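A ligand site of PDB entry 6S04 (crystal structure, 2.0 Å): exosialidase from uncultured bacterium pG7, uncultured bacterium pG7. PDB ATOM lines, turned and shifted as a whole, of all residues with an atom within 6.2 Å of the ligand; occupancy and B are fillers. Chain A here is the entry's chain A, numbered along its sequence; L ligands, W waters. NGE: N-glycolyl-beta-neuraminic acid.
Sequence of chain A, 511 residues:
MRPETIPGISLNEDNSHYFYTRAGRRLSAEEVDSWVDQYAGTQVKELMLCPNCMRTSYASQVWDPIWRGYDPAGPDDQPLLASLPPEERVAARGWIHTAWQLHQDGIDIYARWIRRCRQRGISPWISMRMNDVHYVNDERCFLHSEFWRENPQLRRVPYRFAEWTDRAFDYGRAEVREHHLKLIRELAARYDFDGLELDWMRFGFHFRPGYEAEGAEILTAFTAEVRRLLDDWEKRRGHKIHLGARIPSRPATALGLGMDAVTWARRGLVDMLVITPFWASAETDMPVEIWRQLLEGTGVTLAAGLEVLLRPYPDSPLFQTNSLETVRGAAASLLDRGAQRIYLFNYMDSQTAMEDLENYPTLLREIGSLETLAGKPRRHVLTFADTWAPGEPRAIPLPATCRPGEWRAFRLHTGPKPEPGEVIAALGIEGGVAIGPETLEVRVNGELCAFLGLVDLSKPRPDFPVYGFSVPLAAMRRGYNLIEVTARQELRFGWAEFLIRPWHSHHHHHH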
ATOM      1  N   ASP A  14      15.183 -12.501 -18.298  1.00  0.00           N
ATOM      2  CA  ASP A  14      14.103 -13.305 -18.957  1.00  0.00           C
ATOM      3  C   ASP A  14      13.849 -12.881 -20.430  1.00  0.00           C
ATOM      4  O   ASP A  14      14.453 -11.905 -20.922  1.00  0.00           O
ATOM      5  CB  ASP A  14      12.810 -13.242 -18.133  1.00  0.00           C
ATOM      6  CG  ASP A  14      11.866 -12.070 -18.362  1.00  0.00           C
ATOM      7  OD1 ASP A  14      12.028 -11.345 -19.349  1.00  0.00           O
ATOM      8  OD2 ASP A  14      10.925 -11.900 -17.528  1.00  0.00           O
ATOM      9  N   ASN A  15      12.967 -13.607 -21.107  1.00  0.00           N
ATOM     10  CA  ASN A  15      12.738 -13.563 -22.567  1.00  0.00           C
ATOM     11  C   ASN A  15      11.904 -12.345 -22.973  1.00  0.00           C
ATOM     12  O   ASN A  15      11.800 -12.166 -24.167  1.00  0.00           O
ATOM     13  CB  ASN A  15      12.049 -14.859 -23.061  1.00  0.00           C
ATOM     14  CG  ASN A  15      10.763 -15.129 -22.288  1.00  0.00           C
ATOM     15  OD1 ASN A  15      10.822 -15.298 -21.073  1.00  0.00           O
ATOM     16  ND2 ASN A  15       9.574 -15.048 -22.939  1.00  0.00           N
ATOM     17  N   SER A  16      11.217 -11.657 -22.041  1.00  0.00           N
ATOM     18  CA  SER A  16      10.136 -10.666 -22.366  1.00  0.00           C
ATOM     19  C   SER A  16      10.390  -9.270 -21.795  1.00  0.00           C
ATOM     20  O   SER A  16      10.047  -8.278 -22.465  1.00  0.00           O
ATOM     21  CB  SER A  16       8.775 -11.181 -21.916  1.00  0.00           C
ATOM     22  OG  SER A  16       8.799 -11.475 -20.546  1.00  0.00           O
ATOM     23  N   HIS A  17      10.908  -9.202 -20.566  1.00  0.00           N
ATOM     24  CA  HIS A  17      11.111  -7.975 -19.752  1.00  0.00           C
ATOM     25  C   HIS A  17      11.640  -6.775 -20.570  1.00  0.00           C
ATOM     26  O   HIS A  17      11.092  -5.672 -20.354  1.00  0.00           O
ATOM     27  CB  HIS A  17      12.074  -8.236 -18.593  1.00  0.00           C
ATOM     28  CG  HIS A  17      12.690  -6.995 -18.036  1.00  0.00           C
ATOM     29  ND1 HIS A  17      14.011  -6.657 -18.289  1.00  0.00           N
ATOM     30  CD2 HIS A  17      12.200  -6.030 -17.199  1.00  0.00           C
ATOM     31  CE1 HIS A  17      14.292  -5.507 -17.664  1.00  0.00           C
ATOM     32  NE2 HIS A  17      13.199  -5.114 -16.977  1.00  0.00           N
ATOM     33  N   TYR A  20       9.014  -5.526 -23.081  1.00  0.00           N
ATOM     34  CA  TYR A  20       7.841  -4.908 -22.406  1.00  0.00           C
ATOM     35  C   TYR A  20       8.207  -3.470 -21.953  1.00  0.00           C
ATOM     36  O   TYR A  20       7.432  -2.543 -22.210  1.00  0.00           O
ATOM     37  CB  TYR A  20       7.385  -5.736 -21.203  1.00  0.00           C
ATOM     38  CG  TYR A  20       6.497  -6.951 -21.382  1.00  0.00           C
ATOM     39  CD1 TYR A  20       5.277  -6.887 -22.021  1.00  0.00           C
ATOM     40  CD2 TYR A  20       6.809  -8.143 -20.734  1.00  0.00           C
ATOM     41  CE1 TYR A  20       4.430  -7.978 -22.069  1.00  0.00           C
ATOM     42  CE2 TYR A  20       5.970  -9.250 -20.781  1.00  0.00           C
ATOM     43  CZ  TYR A  20       4.770  -9.163 -21.461  1.00  0.00           C
ATOM     44  OH  TYR A  20       3.932 -10.244 -21.567  1.00  0.00           O
ATOM     45  N   ASN A  52      13.770 -17.070 -25.293  1.00  0.00           N
ATOM     46  CA  ASN A  52      12.655 -17.925 -25.753  1.00  0.00           C
ATOM     47  C   ASN A  52      11.651 -18.189 -24.624  1.00  0.00           C
ATOM     48  O   ASN A  52      12.054 -18.327 -23.430  1.00  0.00           O
ATOM     49  CB  ASN A  52      13.129 -19.232 -26.412  1.00  0.00           C
ATOM     50  CG  ASN A  52      13.467 -20.326 -25.403  1.00  0.00           C
ATOM     51  OD1 ASN A  52      14.478 -20.236 -24.681  1.00  0.00           O
ATOM     52  ND2 ASN A  52      12.579 -21.322 -25.312  1.00  0.00           N
ATOM     53  N   CYS A  53      10.385 -18.331 -25.019  1.00  0.00           N
ATOM     54  CA  CYS A  53       9.386 -19.176 -24.324  1.00  0.00           C
ATOM     55  C   CYS A  53       9.034 -20.292 -25.326  1.00  0.00           C
ATOM     56  O   CYS A  53       9.967 -20.966 -25.836  1.00  0.00           O
ATOM     57  CB  CYS A  53       8.280 -18.265 -23.764  1.00  0.00           C
ATOM     58  SG  CYS A  53       7.578 -17.124 -25.013  1.00  0.00           S
ATOM     59  N   MET A  54       7.753 -20.362 -25.686  1.00  0.00           N
ATOM     60  CA  MET A  54       7.290 -21.284 -26.756  1.00  0.00           C
ATOM     61  C   MET A  54       7.696 -20.637 -28.083  1.00  0.00           C
ATOM     62  O   MET A  54       7.719 -21.346 -29.114  1.00  0.00           O
ATOM     63  CB  MET A  54       5.768 -21.460 -26.681  1.00  0.00           C
ATOM     64  CG  MET A  54       5.323 -22.451 -25.624  1.00  0.00           C
ATOM     65  SD  MET A  54       3.763 -23.480 -26.224  1.00  0.00           S
ATOM     66  CE  MET A  54       2.913 -24.355 -24.682  1.00  0.00           C
ATOM     67  N   TRP A  95       5.894  -5.976 -26.154  1.00  0.00           N
ATOM     68  CA  TRP A  95       6.881  -7.074 -26.340  1.00  0.00           C
ATOM     69  C   TRP A  95       7.004  -7.393 -27.837  1.00  0.00           C
ATOM     70  O   TRP A  95       8.087  -7.218 -28.395  1.00  0.00           O
ATOM     71  CB  TRP A  95       6.521  -8.273 -25.419  1.00  0.00           C
ATOM     72  CG  TRP A  95       7.247  -9.576 -25.640  1.00  0.00           C
ATOM     73  CD1 TRP A  95       8.364  -9.787 -26.386  1.00  0.00           C
ATOM     74  CD2 TRP A  95       6.920 -10.847 -25.061  1.00  0.00           C
ATOM     75  NE1 TRP A  95       8.756 -11.101 -26.350  1.00  0.00           N
ATOM     76  CE2 TRP A  95       7.872 -11.783 -25.526  1.00  0.00           C
ATOM     77  CE3 TRP A  95       5.936 -11.292 -24.174  1.00  0.00           C
ATOM     78  CZ2 TRP A  95       7.843 -13.139 -25.163  1.00  0.00           C
ATOM     79  CZ3 TRP A  95       5.890 -12.631 -23.832  1.00  0.00           C
ATOM     80  CH2 TRP A  95       6.826 -13.552 -24.343  1.00  0.00           C
ATOM     81  N   ARG A 129      14.612 -21.714 -21.993  1.00  0.00           N
ATOM     82  CA  ARG A 129      13.393 -22.219 -21.306  1.00  0.00           C
ATOM     83  C   ARG A 129      13.038 -23.505 -22.057  1.00  0.00           C
ATOM     84  O   ARG A 129      12.810 -23.425 -23.281  1.00  0.00           O
ATOM     85  CB  ARG A 129      12.258 -21.195 -21.391  1.00  0.00           C
ATOM     86  CG  ARG A 129      12.567 -19.871 -20.711  1.00  0.00           C
ATOM     87  CD  ARG A 129      11.319 -19.206 -20.152  1.00  0.00           C
ATOM     88  NE  ARG A 129      11.632 -18.064 -19.302  1.00  0.00           N
ATOM     89  CZ  ARG A 129      10.759 -17.465 -18.494  1.00  0.00           C
ATOM     90  NH1 ARG A 129       9.514 -17.907 -18.422  1.00  0.00           N
ATOM     91  NH2 ARG A 129      11.135 -16.432 -17.776  1.00  0.00           N
ATOM     92  N   ASP A 132       8.182 -23.905 -21.243  1.00  0.00           N
ATOM     93  CA  ASP A 132       7.346 -22.782 -20.756  1.00  0.00           C
ATOM     94  C   ASP A 132       5.873 -23.032 -21.111  1.00  0.00           C
ATOM     95  O   ASP A 132       5.590 -23.494 -22.224  1.00  0.00           O
ATOM     96  CB  ASP A 132       7.844 -21.438 -21.264  1.00  0.00           C
ATOM     97  CG  ASP A 132       7.372 -20.310 -20.363  1.00  0.00           C
ATOM     98  OD1 ASP A 132       6.300 -19.832 -20.544  1.00  0.00           O
ATOM     99  OD2 ASP A 132       8.077 -20.029 -19.418  1.00  0.00           O
ATOM    100  N   HIS A 134       3.245 -20.569 -19.809  1.00  0.00           N
ATOM    101  CA  HIS A 134       2.425 -19.358 -19.504  1.00  0.00           C
ATOM    102  C   HIS A 134       1.140 -19.342 -20.341  1.00  0.00           C
ATOM    103  O   HIS A 134       1.251 -19.404 -21.588  1.00  0.00           O
ATOM    104  CB  HIS A 134       3.187 -18.068 -19.744  1.00  0.00           C
ATOM    105  CG  HIS A 134       4.105 -17.701 -18.639  1.00  0.00           C
ATOM    106  ND1 HIS A 134       5.417 -18.065 -18.672  1.00  0.00           N
ATOM    107  CD2 HIS A 134       3.928 -16.972 -17.511  1.00  0.00           C
ATOM    108  CE1 HIS A 134       6.011 -17.615 -17.558  1.00  0.00           C
ATOM    109  NE2 HIS A 134       5.105 -16.939 -16.815  1.00  0.00           N
ATOM    110  N   TYR A 135      -0.031 -19.319 -19.699  1.00  0.00           N
ATOM    111  CA  TYR A 135      -1.363 -18.979 -20.273  1.00  0.00           C
ATOM    112  C   TYR A 135      -1.862 -20.061 -21.244  1.00  0.00           C
ATOM    113  O   TYR A 135      -2.725 -19.724 -22.115  1.00  0.00           O
ATOM    114  CB  TYR A 135      -1.389 -17.605 -20.968  1.00  0.00           C
ATOM    115  CG  TYR A 135      -0.629 -16.511 -20.267  1.00  0.00           C
ATOM    116  CD1 TYR A 135      -1.004 -15.995 -19.030  1.00  0.00           C
ATOM    117  CD2 TYR A 135       0.461 -15.943 -20.899  1.00  0.00           C
ATOM    118  CE1 TYR A 135      -0.255 -14.989 -18.412  1.00  0.00           C
ATOM    119  CE2 TYR A 135       1.196 -14.913 -20.322  1.00  0.00           C
ATOM    120  CZ  TYR A 135       0.854 -14.443 -19.064  1.00  0.00           C
ATOM    121  OH  TYR A 135       1.664 -13.435 -18.560  1.00  0.00           O
ATOM    122  N   LEU A 143       1.774 -16.205 -27.508  1.00  0.00           N
ATOM    123  CA  LEU A 143       3.150 -16.647 -27.164  1.00  0.00           C
ATOM    124  C   LEU A 143       3.293 -18.175 -27.232  1.00  0.00           C
ATOM    125  O   LEU A 143       4.405 -18.618 -26.826  1.00  0.00           O
ATOM    126  CB  LEU A 143       3.553 -16.132 -25.783  1.00  0.00           C
ATOM    127  CG  LEU A 143       2.566 -16.275 -24.624  1.00  0.00           C
ATOM    128  CD1 LEU A 143       2.300 -17.697 -24.235  1.00  0.00           C
ATOM    129  CD2 LEU A 143       3.096 -15.535 -23.418  1.00  0.00           C
ATOM    130  N   ARG A 202      11.614 -23.895 -15.982  1.00  0.00           N
ATOM    131  CA  ARG A 202      10.415 -23.401 -16.606  1.00  0.00           C
ATOM    132  C   ARG A 202       9.767 -24.543 -17.432  1.00  0.00           C
ATOM    133  O   ARG A 202      10.154 -24.731 -18.601  1.00  0.00           O
ATOM    134  CB  ARG A 202      10.841 -22.156 -17.401  1.00  0.00           C
ATOM    135  CG  ARG A 202      11.108 -20.914 -16.551  1.00  0.00           C
ATOM    136  CD  ARG A 202       9.785 -20.438 -15.969  1.00  0.00           C
ATOM    137  NE  ARG A 202       9.820 -19.373 -14.979  1.00  0.00           N
ATOM    138  CZ  ARG A 202      10.261 -19.567 -13.721  1.00  0.00           C
ATOM    139  NH1 ARG A 202      10.733 -20.736 -13.376  1.00  0.00           N
ATOM    140  NH2 ARG A 202      10.234 -18.583 -12.831  1.00  0.00           N
ATOM    141  N   PHE A 203       8.805 -25.308 -16.870  1.00  0.00           N
ATOM    142  CA  PHE A 203       8.175 -25.081 -15.564  1.00  0.00           C
ATOM    143  C   PHE A 203       8.496 -26.265 -14.626  1.00  0.00           C
ATOM    144  O   PHE A 203       7.782 -26.340 -13.612  1.00  0.00           O
ATOM    145  CB  PHE A 203       6.656 -24.887 -15.611  1.00  0.00           C
ATOM    146  CG  PHE A 203       6.153 -23.489 -15.862  1.00  0.00           C
ATOM    147  CD1 PHE A 203       6.671 -22.714 -16.899  1.00  0.00           C
ATOM    148  CD2 PHE A 203       5.115 -22.973 -15.085  1.00  0.00           C
ATOM    149  CE1 PHE A 203       6.181 -21.446 -17.134  1.00  0.00           C
ATOM    150  CE2 PHE A 203       4.638 -21.684 -15.300  1.00  0.00           C
ATOM    151  CZ  PHE A 203       5.157 -20.941 -16.345  1.00  0.00           C
ATOM    152  N   PHE A 278      10.831 -22.898  -8.338  1.00  0.00           N
ATOM    153  CA  PHE A 278      10.106 -22.467  -9.546  1.00  0.00           C
ATOM    154  C   PHE A 278       9.819 -20.957  -9.490  1.00  0.00           C
ATOM    155  O   PHE A 278      10.355 -20.227 -10.391  1.00  0.00           O
ATOM    156  CB  PHE A 278       8.849 -23.346  -9.664  1.00  0.00           C
ATOM    157  CG  PHE A 278       7.726 -22.820 -10.509  1.00  0.00           C
ATOM    158  CD1 PHE A 278       7.939 -22.596 -11.864  1.00  0.00           C
ATOM    159  CD2 PHE A 278       6.459 -22.649  -9.979  1.00  0.00           C
ATOM    160  CE1 PHE A 278       6.922 -22.103 -12.654  1.00  0.00           C
ATOM    161  CE2 PHE A 278       5.439 -22.104 -10.751  1.00  0.00           C
ATOM    162  CZ  PHE A 278       5.702 -21.775 -12.072  1.00  0.00           C
ATOM    163  N   TRP A 279       9.078 -20.466  -8.487  1.00  0.00           N
ATOM    164  CA  TRP A 279       8.485 -19.090  -8.579  1.00  0.00           C
ATOM    165  C   TRP A 279       7.868 -18.523  -7.283  1.00  0.00           C
ATOM    166  O   TRP A 279       8.031 -17.296  -6.984  1.00  0.00           O
ATOM    167  CB  TRP A 279       7.358 -19.120  -9.589  1.00  0.00           C
ATOM    168  CG  TRP A 279       6.850 -17.743  -9.815  1.00  0.00           C
ATOM    169  CD1 TRP A 279       7.514 -16.733 -10.439  1.00  0.00           C
ATOM    170  CD2 TRP A 279       5.566 -17.227  -9.439  1.00  0.00           C
ATOM    171  NE1 TRP A 279       6.738 -15.616 -10.490  1.00  0.00           N
ATOM    172  CE2 TRP A 279       5.532 -15.874  -9.868  1.00  0.00           C
ATOM    173  CE3 TRP A 279       4.459 -17.731  -8.752  1.00  0.00           C
ATOM    174  CZ2 TRP A 279       4.441 -15.046  -9.636  1.00  0.00           C
ATOM    175  CZ3 TRP A 279       3.377 -16.905  -8.549  1.00  0.00           C
ATOM    176  CH2 TRP A 279       3.368 -15.585  -8.980  1.00  0.00           C
ATOM    177  N   GLU A 307      14.500 -16.674  -6.040  1.00  0.00           N
ATOM    178  CA  GLU A 307      13.378 -16.025  -6.767  1.00  0.00           C
ATOM    179  C   GLU A 307      13.034 -14.705  -6.047  1.00  0.00           C
ATOM    180  O   GLU A 307      13.416 -14.548  -4.891  1.00  0.00           O
ATOM    181  CB  GLU A 307      12.170 -16.951  -6.903  1.00  0.00           C
ATOM    182  CG  GLU A 307      12.145 -17.682  -8.231  1.00  0.00           C
ATOM    183  CD  GLU A 307      11.582 -16.969  -9.437  1.00  0.00           C
ATOM    184  OE1 GLU A 307      11.260 -15.738  -9.351  1.00  0.00           O
ATOM    185  OE2 GLU A 307      11.346 -17.684 -10.447  1.00  0.00           O
ATOM    186  N   PHE A 345      17.158 -15.073 -10.358  1.00  0.00           N
ATOM    187  CA  PHE A 345      16.109 -15.116 -11.414  1.00  0.00           C
ATOM    188  C   PHE A 345      15.075 -14.073 -10.981  1.00  0.00           C
ATOM    189  O   PHE A 345      14.914 -13.900  -9.724  1.00  0.00           O
ATOM    190  CB  PHE A 345      15.508 -16.523 -11.508  1.00  0.00           C
ATOM    191  CG  PHE A 345      14.712 -16.778 -12.768  1.00  0.00           C
ATOM    192  CD1 PHE A 345      13.374 -16.444 -12.852  1.00  0.00           C
ATOM    193  CD2 PHE A 345      15.321 -17.356 -13.875  1.00  0.00           C
ATOM    194  CE1 PHE A 345      12.651 -16.683 -14.006  1.00  0.00           C
ATOM    195  CE2 PHE A 345      14.599 -17.595 -15.029  1.00  0.00           C
ATOM    196  CZ  PHE A 345      13.258 -17.255 -15.096  1.00  0.00           C
ATOM    197  N   ASN A 346      14.547 -13.328 -11.950  1.00  0.00           N
ATOM    198  CA  ASN A 346      13.463 -12.334 -11.781  1.00  0.00           C
ATOM    199  C   ASN A 346      13.943 -11.118 -10.990  1.00  0.00           C
ATOM    200  O   ASN A 346      13.072 -10.319 -10.476  1.00  0.00           O
ATOM    201  CB  ASN A 346      12.228 -13.006 -11.149  1.00  0.00           C
ATOM    202  CG  ASN A 346      11.371 -13.684 -12.191  1.00  0.00           C
ATOM    203  OD1 ASN A 346      11.414 -13.330 -13.392  1.00  0.00           O
ATOM    204  ND2 ASN A 346      10.605 -14.643 -11.745  1.00  0.00           N
ATOM    205  N   MET A 348      15.374  -8.030 -12.048  1.00  0.00           N
ATOM    206  CA  MET A 348      15.696  -7.266 -13.244  1.00  0.00           C
ATOM    207  C   MET A 348      15.662  -5.757 -12.946  1.00  0.00           C
ATOM    208  O   MET A 348      15.358  -5.377 -11.812  1.00  0.00           O
ATOM    209  CB  MET A 348      14.761  -7.753 -14.354  1.00  0.00           C
ATOM    210  CG  MET A 348      15.262  -9.020 -15.022  1.00  0.00           C
ATOM    211  SD  MET A 348      13.953  -9.846 -16.232  1.00  0.00           S
ATOM    212  CE  MET A 348      12.662 -10.945 -15.170  1.00  0.00           C
ATOM    213  N   GLN A 351      10.056  -3.324 -13.404  1.00  0.00           N
ATOM    214  CA  GLN A 351       8.781  -4.096 -13.562  1.00  0.00           C
ATOM    215  C   GLN A 351       8.837  -5.418 -12.775  1.00  0.00           C
ATOM    216  O   GLN A 351       8.210  -5.460 -11.734  1.00  0.00           O
ATOM    217  CB  GLN A 351       8.497  -4.310 -15.047  1.00  0.00           C
ATOM    218  CG  GLN A 351       7.228  -5.110 -15.330  1.00  0.00           C
ATOM    219  CD  GLN A 351       7.012  -5.287 -16.803  1.00  0.00           C
ATOM    220  OE1 GLN A 351       7.604  -6.152 -17.435  1.00  0.00           O
ATOM    221  NE2 GLN A 351       6.170  -4.438 -17.372  1.00  0.00           N
ATOM    222  N   THR A 352       9.474  -6.484 -13.286  1.00  0.00           N
ATOM    223  CA  THR A 352       9.810  -7.719 -12.538  1.00  0.00           C
ATOM    224  C   THR A 352      11.122  -7.546 -11.756  1.00  0.00           C
ATOM    225  O   THR A 352      12.219  -7.684 -12.333  1.00  0.00           O
ATOM    226  CB  THR A 352       9.893  -8.917 -13.499  1.00  0.00           C
ATOM    227  OG1 THR A 352       8.706  -8.873 -14.304  1.00  0.00           O
ATOM    228  CG2 THR A 352       9.993 -10.218 -12.750  1.00  0.00           C
HETATM  229  O9  NGE L   1       7.527 -15.669 -21.801  1.00  0.00           O
HETATM  230  C9  NGE L   1       6.798 -14.750 -20.901  1.00  0.00           C
HETATM  231  C8  NGE L   1       7.609 -14.583 -19.614  1.00  0.00           C
HETATM  232  O8  NGE L   1       8.912 -14.061 -19.922  1.00  0.00           O
HETATM  233  C7  NGE L   1       6.898 -13.618 -18.598  1.00  0.00           C
HETATM  234  O7  NGE L   1       5.570 -14.050 -18.289  1.00  0.00           O
HETATM  235  C6  NGE L   1       7.719 -13.427 -17.323  1.00  0.00           C
HETATM  236  O6  NGE L   1       7.836 -14.703 -16.673  1.00  0.00           O
HETATM  237  C1  NGE L   1       8.731 -16.107 -15.015  1.00  0.00           C
HETATM  238  O1A NGE L   1       9.005 -16.225 -13.720  1.00  0.00           O
HETATM  239  O1B NGE L   1       8.563 -17.064 -15.732  1.00  0.00           O
HETATM  240  O2  NGE L   1       9.975 -14.558 -16.125  1.00  0.00           O
HETATM  241  C3  NGE L   1       8.297 -13.699 -14.523  1.00  0.00           C
HETATM  242  C4  NGE L   1       7.976 -12.307 -15.088  1.00  0.00           C
HETATM  243  O4  NGE L   1       7.372 -11.455 -14.076  1.00  0.00           O
HETATM  244  C5  NGE L   1       7.064 -12.479 -16.323  1.00  0.00           C
HETATM  245  N5  NGE L   1       6.924 -11.189 -16.958  1.00  0.00           N
HETATM  246  C2  NGE L   1       8.696 -14.741 -15.603  1.00  0.00           C
HETATM  247  C10 NGE L   1       5.925 -10.442 -16.707  1.00  0.00           C
HETATM  248  O10 NGE L   1       4.914 -10.858 -16.095  1.00  0.00           O
HETATM  249  C11 NGE L   1       6.219  -9.043 -17.070  1.00  0.00           C
HETATM  250  O11 NGE L   1       4.977  -8.504 -17.414  1.00  0.00           O
HETATM  251  O   HOH W   1       5.588 -17.665 -22.035  1.00  0.00           O
HETATM  252  O   HOH W   2       3.599 -13.809 -15.320  1.00  0.00           O
HETATM  253  O   HOH W   3       9.150 -10.093 -18.250  1.00  0.00           O
HETATM  254  O   HOH W   4       3.881 -12.074 -19.624  1.00  0.00           O
HETATM  255  O   HOH W   5       9.332  -7.816 -16.388  1.00  0.00           O
HETATM  256  O   HOH W   6       4.394  -6.897 -19.318  1.00  0.00           O
HETATM  257  O   HOH W   7       6.574 -18.599 -14.722  1.00  0.00           O
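The side-chain amide nitrogen of Asn 346 is in hydrogen-bond range of an oxygen (O1A) of the ligand (3.0 Å). SG of Cys 53 sits close to O9 of the ligand (3.5 Å). An oxygen (O2) of the ligand lies within hydrogen-bond range of the side-chain carboxylate of Asp 14, 3.2 Å away. A ring nitrogen (NE2) of His 134 lies within hydrogen-bond range of an oxygen (O7) of the ligand, at 3.3 Å. The guanidinium group of Arg 129 lies within salt-bridge range of an oxygen (O1B) of the ligand, at 3.0 Å. NE of Arg 202 lies within salt-bridge range of O1B of the ligand (2.7 Å). The side-chain hydroxyl (OG) of Ser 16 lies within hydrogen-bond range of an oxygen (O8) of the ligand, 2.7 Å away. OG1 of Thr 352 lies within hydrogen-bond range of O4 of the ligand. An oxygen (O9) of the ligand sits at hydrogen-bond distance from the side-chain amide nitrogen of Asn 15, 2.4 Å away.
The side-chain carboxylate of Glu 307 lies within salt-bridge range of the guanidinium group of Arg 202, at 2.8 Å. The side-chain sulfur of Met 348 is in hydrogen-bond range of the backbone NH of Asp 14. The side-chain sulfur (SG) of Cys 53 sits at hydrogen-bond distance from the side-chain amide nitrogen (ND2) of Asn 15 (3.5 Å). OD1 of Asp 14 lies within hydrogen-bond range of N of His 17 (2.7 Å). The guanidinium group (NH2) of Arg 202 sits at hydrogen-bond distance from the backbone carbonyl oxygen (O) of Phe 278 (2.9 Å). The side-chain carboxylate (OD1) of Asp 14 sits at hydrogen-bond distance from the backbone NH (N) of Ser 16 (2.8 Å). The guanidinium group (NH1) of Arg 129 is in salt-bridge range of the side-chain carboxylate (OD2) of Asp 132 (2.7 Å). The backbone carbonyl oxygen (O) of Arg 129 is in hydrogen-bond range of the side-chain amide nitrogen (ND2) of Asn 52 (2.9 Å).
Tyr 20 touches the ligand. Trp 95 touches the ligand. Tyr 135 touches the ligand (OH to O7, 3.96 Å). CD1 of Trp 279 touches O1A of the ligand, 3.6 Å away. Phe 345 touches the ligand. Gln 351 touches the ligand (OE1 to C11, 3.2 Å). Hydrophobic or aromatic side chains within 4 Å of the ligand: Tyr 20, Trp 95, His 134, Trp 279 and Phe 345.
Water W7 lies within hydrogen-bond range of an oxygen (O1B) of the ligand (2.7 Å), a ring nitrogen (NE2) of His 134 (3.0 Å) and the guanidinium group of Arg 202 (3.3 Å). Water W1 lies within hydrogen-bond range of the side-chain carboxylate of Asp 132 (2.7 Å), an oxygen (O9) of the ligand (2.8 Å), a ring nitrogen (ND1) of His 134 (3.4 Å) and the side-chain sulfur of Cys 53 (3.6 Å). Water W3 lies within hydrogen-bond range of the side-chain carboxylate (OD2) of Asp 14 (2.6 Å), the side-chain hydroxyl (OG) of Ser 16 (2.7 Å), a nitrogen (N5) of the ligand (2.8 Å) and the backbone NH (N) of His 17 (3.0 Å). Water W4 lies within hydrogen-bond range of OH of Tyr 20 (2.7 Å), OH of Tyr 135 (2.8 Å) and O7 of the ligand (2.9 Å). Water W5 lies within hydrogen-bond range of OG1 of Thr 352 (2.4 Å) and OE1 of Gln 351 (2.6 Å).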
